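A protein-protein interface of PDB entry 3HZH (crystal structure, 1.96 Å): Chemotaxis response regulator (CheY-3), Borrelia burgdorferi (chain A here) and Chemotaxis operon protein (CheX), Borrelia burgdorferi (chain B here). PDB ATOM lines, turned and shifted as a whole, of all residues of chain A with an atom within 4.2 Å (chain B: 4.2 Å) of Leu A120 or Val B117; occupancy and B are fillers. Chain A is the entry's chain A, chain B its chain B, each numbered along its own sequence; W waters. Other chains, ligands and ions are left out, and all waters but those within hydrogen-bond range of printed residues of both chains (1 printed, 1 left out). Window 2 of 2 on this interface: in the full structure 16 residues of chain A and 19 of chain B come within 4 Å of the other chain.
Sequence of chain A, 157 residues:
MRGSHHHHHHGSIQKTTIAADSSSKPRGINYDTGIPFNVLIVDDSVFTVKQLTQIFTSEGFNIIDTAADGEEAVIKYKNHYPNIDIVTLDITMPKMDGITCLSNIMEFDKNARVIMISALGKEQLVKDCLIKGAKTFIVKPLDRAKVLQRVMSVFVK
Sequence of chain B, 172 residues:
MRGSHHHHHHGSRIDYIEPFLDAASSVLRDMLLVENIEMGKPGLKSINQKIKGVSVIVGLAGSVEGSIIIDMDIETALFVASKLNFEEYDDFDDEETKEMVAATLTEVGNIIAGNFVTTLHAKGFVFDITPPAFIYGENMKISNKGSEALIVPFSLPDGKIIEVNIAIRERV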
ATOM      1  N   ILE A  91     -20.265  13.772 -26.698  1.00  0.00           N
ATOM      2  CA  ILE A  91     -19.430  14.894 -26.290  1.00  0.00           C
ATOM      3  C   ILE A  91     -19.296  15.977 -27.346  1.00  0.00           C
ATOM      4  O   ILE A  91     -19.674  17.123 -27.111  1.00  0.00           O
ATOM      5  CB  ILE A  91     -18.022  14.420 -25.864  1.00  0.00           C
ATOM      6  CG1 ILE A  91     -18.125  13.639 -24.554  1.00  0.00           C
ATOM      7  CG2 ILE A  91     -17.078  15.621 -25.715  1.00  0.00           C
ATOM      8  CD1 ILE A  91     -16.825  13.046 -24.081  1.00  0.00           C
ATOM      9  N   THR A  92     -18.772  15.619 -28.513  1.00  0.00           N
ATOM     10  CA  THR A  92     -18.582  16.601 -29.569  1.00  0.00           C
ATOM     11  C   THR A  92     -19.912  16.990 -30.178  1.00  0.00           C
ATOM     12  O   THR A  92     -20.549  16.198 -30.857  1.00  0.00           O
ATOM     13  CB  THR A  92     -17.627  16.063 -30.658  1.00  0.00           C
ATOM     14  OG1 THR A  92     -16.390  15.703 -30.038  1.00  0.00           O
ATOM     15  CG2 THR A  92     -17.352  17.125 -31.710  1.00  0.00           C
ATOM     16  N   SER A 118     -19.098   8.456 -26.495  1.00  0.00           N
ATOM     17  CA  SER A 118     -18.383   9.317 -27.435  1.00  0.00           C
ATOM     18  C   SER A 118     -17.231   8.690 -28.210  1.00  0.00           C
ATOM     19  O   SER A 118     -16.706   7.649 -27.832  1.00  0.00           O
ATOM     20  CB  SER A 118     -17.871  10.536 -26.680  1.00  0.00           C
ATOM     21  OG  SER A 118     -16.844  11.217 -27.400  1.00  0.00           O
ATOM     22  N   ALA A 119     -16.846   9.353 -29.297  1.00  0.00           N
ATOM     23  CA  ALA A 119     -15.737   8.919 -30.149  1.00  0.00           C
ATOM     24  C   ALA A 119     -14.423   9.245 -29.450  1.00  0.00           C
ATOM     25  O   ALA A 119     -13.366   8.725 -29.821  1.00  0.00           O
ATOM     26  CB  ALA A 119     -15.786   9.643 -31.486  1.00  0.00           C
ATOM     27  N   LEU A 120     -14.498  10.119 -28.449  1.00  0.00           N
ATOM     28  CA  LEU A 120     -13.315  10.526 -27.693  1.00  0.00           C
ATOM     29  C   LEU A 120     -13.135   9.618 -26.488  1.00  0.00           C
ATOM     30  O   LEU A 120     -14.053   9.446 -25.691  1.00  0.00           O
ATOM     31  CB  LEU A 120     -13.469  11.982 -27.242  1.00  0.00           C
ATOM     32  CG  LEU A 120     -13.528  13.008 -28.378  1.00  0.00           C
ATOM     33  CD1 LEU A 120     -14.025  14.346 -27.845  1.00  0.00           C
ATOM     34  CD2 LEU A 120     -12.148  13.148 -29.013  1.00  0.00           C
ATOM     35  N   GLY A 121     -11.945   9.045 -26.346  1.00  0.00           N
ATOM     36  CA  GLY A 121     -11.723   8.148 -25.229  1.00  0.00           C
ATOM     37  C   GLY A 121     -10.459   8.298 -24.409  1.00  0.00           C
ATOM     38  O   GLY A 121     -10.109   7.363 -23.691  1.00  0.00           O
ATOM     39  N   LYS A 122      -9.772   9.434 -24.498  1.00  0.00           N
ATOM     40  CA  LYS A 122      -8.552   9.620 -23.715  1.00  0.00           C
ATOM     41  C   LYS A 122      -8.953   9.229 -22.294  1.00  0.00           C
ATOM     42  O   LYS A 122     -10.009   9.618 -21.791  1.00  0.00           O
ATOM     43  CB  LYS A 122      -8.068  11.075 -23.778  1.00  0.00           C
ATOM     44  CG  LYS A 122      -6.572  11.229 -24.073  1.00  0.00           C
ATOM     45  CD  LYS A 122      -6.174  12.705 -24.136  1.00  0.00           C
ATOM     46  CE  LYS A 122      -4.667  12.906 -24.128  1.00  0.00           C
ATOM     47  NZ  LYS A 122      -4.240  14.314 -23.919  1.00  0.00           N
ATOM     48  N   LEU A 125      -9.920  11.976 -19.802  1.00  0.00           N
ATOM     49  CA  LEU A 125     -11.205  12.590 -20.117  1.00  0.00           C
ATOM     50  C   LEU A 125     -12.283  11.755 -19.430  1.00  0.00           C
ATOM     51  O   LEU A 125     -13.243  12.293 -18.875  1.00  0.00           O
ATOM     52  CB  LEU A 125     -11.446  12.598 -21.628  1.00  0.00           C
ATOM     53  CG  LEU A 125     -12.751  13.248 -22.098  1.00  0.00           C
ATOM     54  CD1 LEU A 125     -12.692  14.744 -21.848  1.00  0.00           C
ATOM     55  CD2 LEU A 125     -12.959  12.975 -23.580  1.00  0.00           C
ATOM     56  N   PHE A 137     -18.739   5.311 -18.955  1.00  0.00           N
ATOM     57  CA  PHE A 137     -18.367   5.855 -20.256  1.00  0.00           C
ATOM     58  C   PHE A 137     -18.333   4.747 -21.317  1.00  0.00           C
ATOM     59  O   PHE A 137     -17.941   3.621 -21.026  1.00  0.00           O
ATOM     60  CB  PHE A 137     -16.973   6.463 -20.098  1.00  0.00           C
ATOM     61  CG  PHE A 137     -16.615   7.493 -21.116  1.00  0.00           C
ATOM     62  CD1 PHE A 137     -16.594   8.842 -20.767  1.00  0.00           C
ATOM     63  CD2 PHE A 137     -16.228   7.122 -22.396  1.00  0.00           C
ATOM     64  CE1 PHE A 137     -16.183   9.805 -21.672  1.00  0.00           C
ATOM     65  CE2 PHE A 137     -15.816   8.079 -23.311  1.00  0.00           C
ATOM     66  CZ  PHE A 137     -15.792   9.422 -22.945  1.00  0.00           C
ATOM     67  N   ALA B 113     -11.770  10.613 -36.469  1.00  0.00           N
ATOM     68  CA  ALA B 113     -11.078  11.735 -35.838  1.00  0.00           C
ATOM     69  C   ALA B 113     -10.941  11.603 -34.324  1.00  0.00           C
ATOM     70  O   ALA B 113      -9.893  11.928 -33.767  1.00  0.00           O
ATOM     71  CB  ALA B 113     -11.782  13.041 -36.172  1.00  0.00           C
ATOM     72  N   GLY B 114     -11.998  11.135 -33.666  1.00  0.00           N
ATOM     73  CA  GLY B 114     -11.964  10.978 -32.226  1.00  0.00           C
ATOM     74  C   GLY B 114     -10.988   9.899 -31.797  1.00  0.00           C
ATOM     75  O   GLY B 114     -10.184  10.102 -30.881  1.00  0.00           O
ATOM     76  N   ASN B 115     -11.061   8.742 -32.446  1.00  0.00           N
ATOM     77  CA  ASN B 115     -10.149   7.658 -32.129  1.00  0.00           C
ATOM     78  C   ASN B 115      -8.726   8.102 -32.428  1.00  0.00           C
ATOM     79  O   ASN B 115      -7.790   7.750 -31.700  1.00  0.00           O
ATOM     80  CB  ASN B 115     -10.512   6.403 -32.926  1.00  0.00           C
ATOM     81  CG  ASN B 115     -11.337   5.422 -32.116  1.00  0.00           C
ATOM     82  OD1 ASN B 115     -12.176   4.694 -32.650  1.00  0.00           O
ATOM     83  ND2 ASN B 115     -11.099   5.397 -30.814  1.00  0.00           N
ATOM     84  N   PHE B 116      -8.565   8.889 -33.489  1.00  0.00           N
ATOM     85  CA  PHE B 116      -7.248   9.399 -33.861  1.00  0.00           C
ATOM     86  C   PHE B 116      -6.654  10.284 -32.754  1.00  0.00           C
ATOM     87  O   PHE B 116      -5.576   9.995 -32.226  1.00  0.00           O
ATOM     88  CB  PHE B 116      -7.334  10.198 -35.164  1.00  0.00           C
ATOM     89  CG  PHE B 116      -6.081  10.963 -35.487  1.00  0.00           C
ATOM     90  CD1 PHE B 116      -4.883  10.295 -35.744  1.00  0.00           C
ATOM     91  CD2 PHE B 116      -6.092  12.355 -35.503  1.00  0.00           C
ATOM     92  CE1 PHE B 116      -3.710  11.006 -36.014  1.00  0.00           C
ATOM     93  CE2 PHE B 116      -4.929  13.079 -35.768  1.00  0.00           C
ATOM     94  CZ  PHE B 116      -3.731  12.401 -36.026  1.00  0.00           C
ATOM     95  N   VAL B 117      -7.348  11.359 -32.390  1.00  0.00           N
ATOM     96  CA  VAL B 117      -6.818  12.232 -31.351  1.00  0.00           C
ATOM     97  C   VAL B 117      -6.697  11.521 -30.001  1.00  0.00           C
ATOM     98  O   VAL B 117      -5.911  11.935 -29.148  1.00  0.00           O
ATOM     99  CB  VAL B 117      -7.663  13.524 -31.183  1.00  0.00           C
ATOM    100  CG1 VAL B 117      -7.650  14.313 -32.474  1.00  0.00           C
ATOM    101  CG2 VAL B 117      -9.088  13.183 -30.773  1.00  0.00           C
ATOM    102  N   THR B 118      -7.463  10.451 -29.806  1.00  0.00           N
ATOM    103  CA  THR B 118      -7.403   9.710 -28.551  1.00  0.00           C
ATOM    104  C   THR B 118      -6.088   8.933 -28.427  1.00  0.00           C
ATOM    105  O   THR B 118      -5.511   8.846 -27.347  1.00  0.00           O
ATOM    106  CB  THR B 118      -8.597   8.732 -28.415  1.00  0.00           C
ATOM    107  OG1 THR B 118      -9.819   9.479 -28.351  1.00  0.00           O
ATOM    108  CG2 THR B 118      -8.467   7.887 -27.144  1.00  0.00           C
ATOM    109  N   THR B 119      -5.611   8.378 -29.535  1.00  0.00           N
ATOM    110  CA  THR B 119      -4.368   7.623 -29.508  1.00  0.00           C
ATOM    111  C   THR B 119      -3.219   8.603 -29.392  1.00  0.00           C
ATOM    112  O   THR B 119      -2.047   8.236 -29.487  1.00  0.00           O
ATOM    113  CB  THR B 119      -4.193   6.776 -30.777  1.00  0.00           C
ATOM    114  OG1 THR B 119      -4.167   7.629 -31.923  1.00  0.00           O
ATOM    115  CG2 THR B 119      -5.344   5.793 -30.914  1.00  0.00           C
ATOM    116  N   LEU B 120      -3.562   9.869 -29.189  1.00  0.00           N
ATOM    117  CA  LEU B 120      -2.540  10.875 -29.042  1.00  0.00           C
ATOM    118  C   LEU B 120      -2.141  11.184 -27.602  1.00  0.00           C
ATOM    119  O   LEU B 120      -1.246  12.006 -27.401  1.00  0.00           O
ATOM    120  CB  LEU B 120      -2.912  12.141 -29.820  1.00  0.00           C
ATOM    121  CG  LEU B 120      -2.677  11.959 -31.326  1.00  0.00           C
ATOM    122  CD1 LEU B 120      -3.113  13.188 -32.098  1.00  0.00           C
ATOM    123  CD2 LEU B 120      -1.201  11.692 -31.569  1.00  0.00           C
ATOM    124  N   PHE B 127      -5.266  17.440 -27.932  1.00  0.00           N
ATOM    125  CA  PHE B 127      -5.658  17.408 -29.329  1.00  0.00           C
ATOM    126  C   PHE B 127      -7.172  17.349 -29.362  1.00  0.00           C
ATOM    127  O   PHE B 127      -7.764  16.362 -28.932  1.00  0.00           O
ATOM    128  CB  PHE B 127      -5.055  16.181 -30.018  1.00  0.00           C
ATOM    129  CG  PHE B 127      -3.615  15.922 -29.647  1.00  0.00           C
ATOM    130  CD1 PHE B 127      -3.297  15.108 -28.562  1.00  0.00           C
ATOM    131  CD2 PHE B 127      -2.575  16.517 -30.361  1.00  0.00           C
ATOM    132  CE1 PHE B 127      -1.963  14.885 -28.190  1.00  0.00           C
ATOM    133  CE2 PHE B 127      -1.239  16.302 -29.995  1.00  0.00           C
ATOM    134  CZ  PHE B 127      -0.937  15.484 -28.910  1.00  0.00           C
ATOM    135  N   ILE B 129     -11.069  18.108 -31.480  1.00  0.00           N
ATOM    136  CA  ILE B 129     -11.700  18.035 -32.792  1.00  0.00           C
ATOM    137  C   ILE B 129     -12.965  18.888 -32.766  1.00  0.00           C
ATOM    138  O   ILE B 129     -13.463  19.237 -31.705  1.00  0.00           O
ATOM    139  CB  ILE B 129     -12.068  16.578 -33.189  1.00  0.00           C
ATOM    140  CG1 ILE B 129     -13.109  16.002 -32.229  1.00  0.00           C
ATOM    141  CG2 ILE B 129     -10.813  15.702 -33.171  1.00  0.00           C
ATOM    142  CD1 ILE B 129     -13.543  14.581 -32.607  1.00  0.00           C
HETATM  143  O   HOH W   1     -10.091  11.476 -26.144  1.00  0.00           O
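Printed residues of chain B that touch a printed residue of chain A: Gly B114, Asn B115, Val B117, Thr B118 and Ile B129. Hydrophobic or aromatic side chains of chain B that line the printed part of chain A: Val B117 and Ile B129. Hydrophobic or aromatic side chains of chain A that line the printed part of chain B: Leu A120. Along chain A the printed residues that touch a printed residue of chain B span positions 92 to 122. Among the printed residues, 9 pairs touch across the chains.
The side-chain hydroxyl (OG) of Ser A118 is in hydrogen-bond range of the backbone NH (N) of Leu A120. OG1 of Thr B118 is in hydrogen-bond range of O of Gly B114 (2.6 Å).
O of Ala A119 lies within hydrogen-bond range of N of Asn B115, 3.5 Å away. The side-chain hydroxyl (OG1) of Thr B118 sits at hydrogen-bond distance from the backbone NH (N) of Gly A121 (3.0 Å).
Among the printed residues, pairs that only touch across the chains: Thr A92 with Ile B129 (3.96 Å), Ala A119 with Gly B114 (3.3 Å), Ala A119 with Thr B118 (3.9 Å), Leu A120 with Gly B114 (3.9 Å), Leu A120 with Val B117 (3.5 Å), Leu A120 with Thr B118 (3.7 Å) and Lys A122 with Thr B118 (3.3 Å).
Water W1 lies within hydrogen-bond range of N of Lys A122 (2.6 Å), OG1 of Thr B118 (3.0 Å) and N of Gly A121 (3.1 Å).
Of the printed residues of chain B, Thr A92 touches Ile B129. Of the printed residues of chain B, Leu A120 touches Gly B114 (3.9 Å), Val B117 (3.5 Å) and Thr B118 (3.7 Å). Printed residues of chain B within 4 Å of Gly A121: Thr B118 (3.0 Å). Printed residues of chain B within 4 Å of Lys A122: Thr B118. Ala B113 touches none of the printed residues of chain A. Printed residues of chain A within 4 Å of Gly B114: Ala A119 and Leu A120. Of the printed residues of chain A, Asn B115 touches Ala A119 (3.5 Å). Of chain A, only Leu A120 comes within 4 Å of Val B117. Leu B120 touches none of the printed residues of chain A. The nearest printed residue of chain A that does not touch Asn B115 is Leu A120 (5.4 Å).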
